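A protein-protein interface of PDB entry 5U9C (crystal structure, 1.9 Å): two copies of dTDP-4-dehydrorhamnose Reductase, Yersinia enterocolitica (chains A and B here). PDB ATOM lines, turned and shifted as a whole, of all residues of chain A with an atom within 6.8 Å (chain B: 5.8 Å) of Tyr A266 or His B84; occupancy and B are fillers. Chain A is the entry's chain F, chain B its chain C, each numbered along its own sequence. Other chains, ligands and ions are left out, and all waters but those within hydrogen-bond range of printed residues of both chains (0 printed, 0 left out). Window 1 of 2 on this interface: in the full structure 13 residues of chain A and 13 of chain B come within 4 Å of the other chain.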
ATOM      1  N   GLU A 120     -16.546   2.513   0.940  1.00  0.00           N
ATOM      2  CA  GLU A 120     -16.651   2.465   2.389  1.00  0.00           C
ATOM      3  C   GLU A 120     -17.878   3.151   3.004  1.00  0.00           C
ATOM      4  O   GLU A 120     -18.181   2.923   4.172  1.00  0.00           O
ATOM      5  CB  GLU A 120     -15.371   2.965   3.056  1.00  0.00           C
ATOM      6  CG  GLU A 120     -14.110   2.140   2.804  1.00  0.00           C
ATOM      7  CD  GLU A 120     -13.293   2.539   1.575  1.00  0.00           C
ATOM      8  OE1 GLU A 120     -13.803   3.256   0.684  1.00  0.00           O
ATOM      9  OE2 GLU A 120     -12.113   2.105   1.505  1.00  0.00           O
ATOM     10  N   LEU A 121     -18.559   4.010   2.253  1.00  0.00           N
ATOM     11  CA  LEU A 121     -19.785   4.653   2.741  1.00  0.00           C
ATOM     12  C   LEU A 121     -21.024   3.804   2.490  1.00  0.00           C
ATOM     13  O   LEU A 121     -22.075   4.062   3.081  1.00  0.00           O
ATOM     14  CB  LEU A 121     -20.002   6.040   2.106  1.00  0.00           C
ATOM     15  CG  LEU A 121     -19.148   7.158   2.645  1.00  0.00           C
ATOM     16  CD1 LEU A 121     -19.421   8.442   1.866  1.00  0.00           C
ATOM     17  CD2 LEU A 121     -19.416   7.353   4.147  1.00  0.00           C
ATOM     18  N   HIS A 211      -2.562   1.789  11.670  1.00  0.00           N
ATOM     19  CA  HIS A 211      -3.699   2.398  10.970  1.00  0.00           C
ATOM     20  C   HIS A 211      -5.010   1.781  11.449  1.00  0.00           C
ATOM     21  O   HIS A 211      -5.060   0.587  11.703  1.00  0.00           O
ATOM     22  CB  HIS A 211      -3.559   2.222   9.455  1.00  0.00           C
ATOM     23  CG  HIS A 211      -4.654   2.883   8.692  1.00  0.00           C
ATOM     24  ND1 HIS A 211      -4.813   4.254   8.670  1.00  0.00           N
ATOM     25  CD2 HIS A 211      -5.662   2.372   7.950  1.00  0.00           C
ATOM     26  CE1 HIS A 211      -5.883   4.558   7.955  1.00  0.00           C
ATOM     27  NE2 HIS A 211      -6.409   3.436   7.495  1.00  0.00           N
ATOM     28  N   THR A 214     -12.005   1.154   8.614  1.00  0.00           N
ATOM     29  CA  THR A 214     -12.441   0.162   7.643  1.00  0.00           C
ATOM     30  C   THR A 214     -11.970   0.655   6.279  1.00  0.00           C
ATOM     31  O   THR A 214     -12.144   1.834   5.938  1.00  0.00           O
ATOM     32  CB  THR A 214     -13.974  -0.057   7.698  1.00  0.00           C
ATOM     33  OG1 THR A 214     -14.311  -0.636   8.961  1.00  0.00           O
ATOM     34  CG2 THR A 214     -14.459  -1.005   6.592  1.00  0.00           C
ATOM     35  N   LEU A 215     -11.379  -0.249   5.511  1.00  0.00           N
ATOM     36  CA  LEU A 215     -10.838   0.082   4.224  1.00  0.00           C
ATOM     37  C   LEU A 215     -11.086  -1.035   3.198  1.00  0.00           C
ATOM     38  O   LEU A 215     -11.019  -2.218   3.529  1.00  0.00           O
ATOM     39  CB  LEU A 215      -9.345   0.281   4.401  1.00  0.00           C
ATOM     40  CG  LEU A 215      -8.494   1.005   3.375  1.00  0.00           C
ATOM     41  CD1 LEU A 215      -8.907   2.470   3.280  1.00  0.00           C
ATOM     42  CD2 LEU A 215      -7.039   0.920   3.830  1.00  0.00           C
ATOM     43  N   HIS A 216     -11.378  -0.632   1.965  1.00  0.00           N
ATOM     44  CA  HIS A 216     -11.527  -1.532   0.860  1.00  0.00           C
ATOM     45  C   HIS A 216     -10.181  -1.601   0.134  1.00  0.00           C
ATOM     46  O   HIS A 216      -9.601  -0.556  -0.206  1.00  0.00           O
ATOM     47  CB  HIS A 216     -12.582  -0.991  -0.086  1.00  0.00           C
ATOM     48  CG  HIS A 216     -13.969  -1.070   0.457  1.00  0.00           C
ATOM     49  ND1 HIS A 216     -15.077  -0.826  -0.319  1.00  0.00           N
ATOM     50  CD2 HIS A 216     -14.436  -1.495   1.661  1.00  0.00           C
ATOM     51  CE1 HIS A 216     -16.167  -1.005   0.413  1.00  0.00           C
ATOM     52  NE2 HIS A 216     -15.804  -1.418   1.614  1.00  0.00           N
ATOM     53  N   GLU A 263     -14.596  -0.517  -4.356  1.00  0.00           N
ATOM     54  CA  GLU A 263     -13.625   0.519  -4.616  1.00  0.00           C
ATOM     55  C   GLU A 263     -13.414   1.296  -3.322  1.00  0.00           C
ATOM     56  O   GLU A 263     -14.212   1.193  -2.384  1.00  0.00           O
ATOM     57  CB  GLU A 263     -14.057   1.416  -5.765  1.00  0.00           C
ATOM     58  CG  GLU A 263     -15.290   2.232  -5.537  1.00  0.00           C
ATOM     59  CD  GLU A 263     -15.800   2.862  -6.832  1.00  0.00           C
ATOM     60  OE1 GLU A 263     -16.030   2.132  -7.803  1.00  0.00           O
ATOM     61  OE2 GLU A 263     -16.024   4.075  -6.857  1.00  0.00           O
ATOM     62  N   SER A 264     -12.324   2.043  -3.254  1.00  0.00           N
ATOM     63  CA  SER A 264     -12.050   2.801  -2.053  1.00  0.00           C
ATOM     64  C   SER A 264     -12.087   4.277  -2.284  1.00  0.00           C
ATOM     65  O   SER A 264     -11.608   4.765  -3.309  1.00  0.00           O
ATOM     66  CB  SER A 264     -10.681   2.450  -1.487  1.00  0.00           C
ATOM     67  OG  SER A 264     -10.483   3.121  -0.240  1.00  0.00           O
ATOM     68  N   ILE A 265     -12.642   4.986  -1.305  1.00  0.00           N
ATOM     69  CA  ILE A 265     -12.641   6.436  -1.305  1.00  0.00           C
ATOM     70  C   ILE A 265     -11.658   6.962  -0.244  1.00  0.00           C
ATOM     71  O   ILE A 265     -11.507   8.183  -0.078  1.00  0.00           O
ATOM     72  CB  ILE A 265     -14.038   7.019  -1.033  1.00  0.00           C
ATOM     73  CG1 ILE A 265     -14.604   6.512   0.304  1.00  0.00           C
ATOM     74  CG2 ILE A 265     -14.975   6.689  -2.200  1.00  0.00           C
ATOM     75  CD1 ILE A 265     -15.888   7.194   0.741  1.00  0.00           C
ATOM     76  N   TYR A 266     -11.028   6.062   0.506  1.00  0.00           N
ATOM     77  CA  TYR A 266     -10.122   6.497   1.576  1.00  0.00           C
ATOM     78  C   TYR A 266      -8.661   6.103   1.388  1.00  0.00           C
ATOM     79  O   TYR A 266      -7.813   6.574   2.127  1.00  0.00           O
ATOM     80  CB  TYR A 266     -10.596   5.972   2.936  1.00  0.00           C
ATOM     81  CG  TYR A 266     -11.963   6.428   3.385  1.00  0.00           C
ATOM     82  CD1 TYR A 266     -12.376   7.740   3.213  1.00  0.00           C
ATOM     83  CD2 TYR A 266     -12.793   5.577   4.127  1.00  0.00           C
ATOM     84  CE1 TYR A 266     -13.611   8.165   3.661  1.00  0.00           C
ATOM     85  CE2 TYR A 266     -14.021   6.019   4.610  1.00  0.00           C
ATOM     86  CZ  TYR A 266     -14.423   7.316   4.373  1.00  0.00           C
ATOM     87  OH  TYR A 266     -15.638   7.782   4.853  1.00  0.00           O
ATOM     88  N   MET A 267      -8.359   5.277   0.398  1.00  0.00           N
ATOM     89  CA  MET A 267      -6.970   4.850   0.172  1.00  0.00           C
ATOM     90  C   MET A 267      -6.040   5.998  -0.193  1.00  0.00           C
ATOM     91  O   MET A 267      -4.872   6.021   0.225  1.00  0.00           O
ATOM     92  CB  MET A 267      -6.995   3.828  -0.959  1.00  0.00           C
ATOM     93  CG  MET A 267      -5.678   3.097  -1.185  1.00  0.00           C
ATOM     94  SD  MET A 267      -5.235   1.913   0.328  1.00  0.00           S
ATOM     95  CE  MET A 267      -6.782   0.725   0.349  1.00  0.00           C
ATOM     96  N   SER A 268      -6.545   6.977  -0.939  1.00  0.00           N
ATOM     97  CA  SER A 268      -5.694   8.075  -1.417  1.00  0.00           C
ATOM     98  C   SER A 268      -5.118   8.990  -0.339  1.00  0.00           C
ATOM     99  O   SER A 268      -4.075   9.592  -0.571  1.00  0.00           O
ATOM    100  CB  SER A 268      -6.411   8.891  -2.490  1.00  0.00           C
ATOM    101  OG  SER A 268      -7.545   9.541  -1.978  1.00  0.00           O
ATOM    102  N   ILE A 269      -5.779   9.117   0.816  1.00  0.00           N
ATOM    103  CA  ILE A 269      -5.206   9.930   1.912  1.00  0.00           C
ATOM    104  C   ILE A 269      -4.121   9.180   2.715  1.00  0.00           C
ATOM    105  O   ILE A 269      -3.573   9.736   3.673  1.00  0.00           O
ATOM    106  CB  ILE A 269      -6.256  10.524   2.891  1.00  0.00           C
ATOM    107  CG1 ILE A 269      -7.086   9.432   3.561  1.00  0.00           C
ATOM    108  CG2 ILE A 269      -7.154  11.511   2.163  1.00  0.00           C
ATOM    109  CD1 ILE A 269      -8.065   9.960   4.592  1.00  0.00           C
ATOM    110  N   LEU A 270      -3.818   7.934   2.334  1.00  0.00           N
ATOM    111  CA  LEU A 270      -2.781   7.160   2.988  1.00  0.00           C
ATOM    112  C   LEU A 270      -1.518   7.351   2.150  1.00  0.00           C
ATOM    113  O   LEU A 270      -1.047   6.456   1.462  1.00  0.00           O
ATOM    114  CB  LEU A 270      -3.209   5.704   3.130  1.00  0.00           C
ATOM    115  CG  LEU A 270      -4.548   5.551   3.859  1.00  0.00           C
ATOM    116  CD1 LEU A 270      -4.819   4.091   4.074  1.00  0.00           C
ATOM    117  CD2 LEU A 270      -4.585   6.286   5.203  1.00  0.00           C
ATOM    118  N   PRO B  76     -17.824  11.197  -3.151  1.00  0.00           N
ATOM    119  CA  PRO B  76     -18.090  10.536  -1.870  1.00  0.00           C
ATOM    120  C   PRO B  76     -16.895  10.568  -0.905  1.00  0.00           C
ATOM    121  O   PRO B  76     -17.092  10.510   0.310  1.00  0.00           O
ATOM    122  CB  PRO B  76     -18.487   9.111  -2.265  1.00  0.00           C
ATOM    123  CG  PRO B  76     -18.077   8.948  -3.694  1.00  0.00           C
ATOM    124  CD  PRO B  76     -18.086  10.323  -4.299  1.00  0.00           C
ATOM    125  N   ALA B  77     -15.677  10.704  -1.428  1.00  0.00           N
ATOM    126  CA  ALA B  77     -14.504  10.784  -0.553  1.00  0.00           C
ATOM    127  C   ALA B  77     -14.603  12.009   0.365  1.00  0.00           C
ATOM    128  O   ALA B  77     -14.259  11.934   1.551  1.00  0.00           O
ATOM    129  CB  ALA B  77     -13.221  10.851  -1.378  1.00  0.00           C
ATOM    130  N   ALA B  79     -17.474  13.590   1.205  1.00  0.00           N
ATOM    131  CA  ALA B  79     -18.582  13.319   2.136  1.00  0.00           C
ATOM    132  C   ALA B  79     -18.100  12.423   3.266  1.00  0.00           C
ATOM    133  O   ALA B  79     -18.400  12.668   4.428  1.00  0.00           O
ATOM    134  CB  ALA B  79     -19.743  12.657   1.413  1.00  0.00           C
ATOM    135  N   GLY B  80     -17.297  11.413   2.930  1.00  0.00           N
ATOM    136  CA  GLY B  80     -16.809  10.479   3.942  1.00  0.00           C
ATOM    137  C   GLY B  80     -15.805  11.105   4.900  1.00  0.00           C
ATOM    138  O   GLY B  80     -15.913  10.978   6.121  1.00  0.00           O
ATOM    139  N   ILE B  81     -14.814  11.787   4.345  1.00  0.00           N
ATOM    140  CA  ILE B  81     -13.799  12.436   5.183  1.00  0.00           C
ATOM    141  C   ILE B  81     -14.423  13.453   6.140  1.00  0.00           C
ATOM    142  O   ILE B  81     -14.141  13.451   7.326  1.00  0.00           O
ATOM    143  CB  ILE B  81     -12.707  13.115   4.323  1.00  0.00           C
ATOM    144  CG1 ILE B  81     -11.870  12.045   3.621  1.00  0.00           C
ATOM    145  CG2 ILE B  81     -11.776  13.952   5.201  1.00  0.00           C
ATOM    146  CD1 ILE B  81     -10.990  12.579   2.509  1.00  0.00           C
ATOM    147  N   TYR B  82     -15.260  14.311   5.598  1.00  0.00           N
ATOM    148  CA  TYR B  82     -15.890  15.404   6.352  1.00  0.00           C
ATOM    149  C   TYR B  82     -16.947  15.008   7.346  1.00  0.00           C
ATOM    150  O   TYR B  82     -16.962  15.556   8.438  1.00  0.00           O
ATOM    151  CB  TYR B  82     -16.531  16.435   5.401  1.00  0.00           C
ATOM    152  CG  TYR B  82     -15.587  17.432   4.758  1.00  0.00           C
ATOM    153  CD1 TYR B  82     -14.430  17.021   4.114  1.00  0.00           C
ATOM    154  CD2 TYR B  82     -15.905  18.787   4.722  1.00  0.00           C
ATOM    155  CE1 TYR B  82     -13.587  17.928   3.499  1.00  0.00           C
ATOM    156  CE2 TYR B  82     -15.053  19.711   4.116  1.00  0.00           C
ATOM    157  CZ  TYR B  82     -13.906  19.270   3.497  1.00  0.00           C
ATOM    158  OH  TYR B  82     -13.059  20.160   2.878  1.00  0.00           O
ATOM    159  N   ASN B  83     -17.855  14.113   6.939  1.00  0.00           N
ATOM    160  CA  ASN B  83     -19.005  13.707   7.751  1.00  0.00           C
ATOM    161  C   ASN B  83     -18.790  12.405   8.554  1.00  0.00           C
ATOM    162  O   ASN B  83     -19.378  12.226   9.631  1.00  0.00           O
ATOM    163  CB  ASN B  83     -20.250  13.582   6.856  1.00  0.00           C
ATOM    164  CG  ASN B  83     -20.649  14.911   6.196  1.00  0.00           C
ATOM    165  OD1 ASN B  83     -20.280  15.986   6.673  1.00  0.00           O
ATOM    166  ND2 ASN B  83     -21.397  14.837   5.076  1.00  0.00           N
ATOM    167  N   HIS B  84     -17.971  11.497   8.031  1.00  0.00           N
ATOM    168  CA  HIS B  84     -17.714  10.237   8.725  1.00  0.00           C
ATOM    169  C   HIS B  84     -16.407  10.249   9.509  1.00  0.00           C
ATOM    170  O   HIS B  84     -16.437  10.211  10.745  1.00  0.00           O
ATOM    171  CB  HIS B  84     -17.813   9.064   7.735  1.00  0.00           C
ATOM    172  CG  HIS B  84     -17.279   7.770   8.248  1.00  0.00           C
ATOM    173  ND1 HIS B  84     -16.737   6.822   7.407  1.00  0.00           N
ATOM    174  CD2 HIS B  84     -17.162   7.277   9.505  1.00  0.00           C
ATOM    175  CE1 HIS B  84     -16.341   5.783   8.124  1.00  0.00           C
ATOM    176  NE2 HIS B  84     -16.581   6.034   9.398  1.00  0.00           N
ATOM    177  N   LEU B  85     -15.266  10.330   8.816  1.00  0.00           N
ATOM    178  CA  LEU B  85     -13.974  10.257   9.511  1.00  0.00           C
ATOM    179  C   LEU B  85     -13.776  11.368  10.532  1.00  0.00           C
ATOM    180  O   LEU B  85     -13.309  11.107  11.636  1.00  0.00           O
ATOM    181  CB  LEU B  85     -12.794  10.208   8.521  1.00  0.00           C
ATOM    182  CG  LEU B  85     -12.817   9.082   7.487  1.00  0.00           C
ATOM    183  CD1 LEU B  85     -11.565   9.118   6.609  1.00  0.00           C
ATOM    184  CD2 LEU B  85     -12.977   7.711   8.156  1.00  0.00           C
ATOM    185  N   ALA B  86     -14.135  12.600  10.184  1.00  0.00           N
ATOM    186  CA  ALA B  86     -13.989  13.695  11.123  1.00  0.00           C
ATOM    187  C   ALA B  86     -14.871  13.469  12.346  1.00  0.00           C
ATOM    188  O   ALA B  86     -14.412  13.635  13.499  1.00  0.00           O
ATOM    189  CB  ALA B  86     -14.301  15.031  10.460  1.00  0.00           C
ATOM    190  N   THR B  87     -16.114  13.065  12.102  1.00  0.00           N
ATOM    191  CA  THR B  87     -17.066  12.781  13.189  1.00  0.00           C
ATOM    192  C   THR B  87     -16.558  11.652  14.109  1.00  0.00           C
ATOM    193  O   THR B  87     -16.656  11.764  15.319  1.00  0.00           O
ATOM    194  CB  THR B  87     -18.461  12.486  12.629  1.00  0.00           C
ATOM    195  OG1 THR B  87     -18.916  13.647  11.908  1.00  0.00           O
ATOM    196  CG2 THR B  87     -19.463  12.164  13.754  1.00  0.00           C
ATOM    197  N   GLU B  88     -15.970  10.607  13.535  1.00  0.00           N
ATOM    198  CA  GLU B  88     -15.395   9.512  14.333  1.00  0.00           C
ATOM    199  C   GLU B  88     -14.316  10.041  15.303  1.00  0.00           C
ATOM    200  O   GLU B  88     -14.302   9.672  16.478  1.00  0.00           O
ATOM    201  CB  GLU B  88     -14.809   8.435  13.408  1.00  0.00           C
ATOM    202  CG  GLU B  88     -13.846   7.434  14.040  1.00  0.00           C
ATOM    203  CD  GLU B  88     -14.476   6.543  15.088  1.00  0.00           C
ATOM    204  OE1 GLU B  88     -15.715   6.449  15.126  1.00  0.00           O
ATOM    205  OE2 GLU B  88     -13.719   5.911  15.871  1.00  0.00           O
ATOM    206  N   GLN B  89     -13.429  10.914  14.812  1.00  0.00           N
ATOM    207  CA  GLN B  89     -12.366  11.484  15.666  1.00  0.00           C
ATOM    208  C   GLN B  89     -12.948  12.401  16.746  1.00  0.00           C
ATOM    209  O   GLN B  89     -12.479  12.391  17.898  1.00  0.00           O
ATOM    210  CB  GLN B  89     -11.289  12.184  14.839  1.00  0.00           C
ATOM    211  CG  GLN B  89     -10.568  11.238  13.887  1.00  0.00           C
ATOM    212  CD  GLN B  89      -9.820  10.164  14.636  1.00  0.00           C
ATOM    213  OE1 GLN B  89      -9.016  10.463  15.493  1.00  0.00           O
ATOM    214  NE2 GLN B  89     -10.097   8.920  14.327  1.00  0.00           N
ATOM    215  N   SER B 133     -23.172   9.137   4.711  1.00  0.00           N
ATOM    216  CA  SER B 133     -22.090   9.743   5.482  1.00  0.00           C
ATOM    217  C   SER B 133     -22.595  10.253   6.842  1.00  0.00           C
ATOM    218  O   SER B 133     -21.911  10.117   7.853  1.00  0.00           O
ATOM    219  CB  SER B 133     -21.353  10.844   4.693  1.00  0.00           C
ATOM    220  OG  SER B 133     -22.124  12.016   4.573  1.00  0.00           O
ATOM    221  N   ILE B 136     -23.349   6.958   9.047  1.00  0.00           N
ATOM    222  CA  ILE B 136     -22.150   6.334   9.582  1.00  0.00           C
ATOM    223  C   ILE B 136     -21.568   7.266  10.673  1.00  0.00           C
ATOM    224  O   ILE B 136     -21.045   6.786  11.690  1.00  0.00           O
ATOM    225  CB  ILE B 136     -21.154   5.920   8.482  1.00  0.00           C
ATOM    226  CG1 ILE B 136     -21.807   4.852   7.594  1.00  0.00           C
ATOM    227  CG2 ILE B 136     -19.922   5.286   9.107  1.00  0.00           C
ATOM    228  CD1 ILE B 136     -21.043   4.505   6.331  1.00  0.00           C
ATOM    229  N   GLY B 137     -21.705   8.584  10.477  1.00  0.00           N
ATOM    230  CA  GLY B 137     -21.340   9.552  11.523  1.00  0.00           C
ATOM    231  C   GLY B 137     -22.116   9.281  12.813  1.00  0.00           C
ATOM    232  O   GLY B 137     -21.520   9.252  13.890  1.00  0.00           O
ATOM    233  N   SER B 140     -20.734   6.236  14.650  1.00  0.00           N
ATOM    234  CA  SER B 140     -19.480   6.558  15.347  1.00  0.00           C
ATOM    235  C   SER B 140     -19.784   7.193  16.686  1.00  0.00           C
ATOM    236  O   SER B 140     -19.141   6.863  17.696  1.00  0.00           O
ATOM    237  CB  SER B 140     -18.632   7.535  14.538  1.00  0.00           C
ATOM    238  OG  SER B 140     -18.216   6.925  13.335  1.00  0.00           O
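O of Gly B80 sits close to OH of Tyr A266, at 3.4 Å. ND1 of His B84 lies within hydrogen-bond range of OH of Tyr A266.
The backbone carbonyl oxygen (O) of Gly B80 sits at hydrogen-bond distance from the backbone NH (N) of Leu B85 (2.8 Å). The backbone carbonyl oxygen (O) of Ile B81 is in hydrogen-bond range of the backbone NH (N) of Ala B86 (3.0 Å). The side-chain amide nitrogen (ND2) of Asn B83 sits at hydrogen-bond distance from the side-chain hydroxyl (OG) of Ser B133 (3.0 Å). OG of Ser B140 lies within hydrogen-bond range of O of Ile B136 (3.3 Å). The backbone NH (N) of His A216 sits at hydrogen-bond distance from the side-chain carboxylate (OE2) of Glu A120. N of Tyr A266 sits at hydrogen-bond distance from OG of Ser A264, 3.1 Å away.
Among the printed residues, merely in contact across the chains: Glu A120 with Ile B136 (3.9 Å), Leu A121 with Pro B76 (3.5 Å), Leu A121 with Gly B80 (3.8 Å), Leu A121 with Ser B133 (3.8 Å), Leu A121 with Ile B136 (3.4 Å), Ile A265 with Pro B76 (3.6 Å), Ile A265 with Ala B77 (3.4 Å), Tyr A266 with Ile B81 (3.9 Å), Tyr A266 with Leu B85 (3.7 Å) and Ile A269 with Ile B81 (3.997 Å).
Printed residues of chain B within 4 Å of Glu A120: Ile B136 (3.9 Å). His A211 touches none of the printed residues of chain B. Of chain B, only Gly B80 (3.1 Å), Ile B81 (3.9 Å), His B84 (2.9 Å) and Leu B85 (3.7 Å) come within 4 Å of Tyr A266. Printed residues of chain A within 4 Å of Gly B80: Leu A121 and Tyr A266. Of the printed residues of chain A, Ile B81 touches Tyr A266 and Ile A269. His B84 touches just one residue of chain A: Tyr A266 (2.9 Å). Of the printed residues of chain A, Leu B85 touches Tyr A266 (3.7 Å). Ala B86 touches none of the printed residues of chain A. The nearest residue of chain B that does not touch Tyr A266 is Ala B77 (4.4 Å). The nearest printed residue of chain A that does not touch Ser B133 is Tyr A266 (6.5 Å).
Of the 14 printed residues of chain A, 5 touch a printed residue of chain B. Hydrophobic or aromatic side chains of chain A that line the printed part of chain B: Leu A121, Ile A265, Tyr A266 and Ile A269. Of the 17 printed residues of chain B, 8 touch a printed residue of chain A. Among the printed residues, no Asp or Glu carboxylate lies within 4 Å of a Lys or Arg side-chain nitrogen of the other chain.
No position is printed for both chains. Of the 12 pairs that touch across the chains among the printed residues, none has its exchanged pair printed and touching as well.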
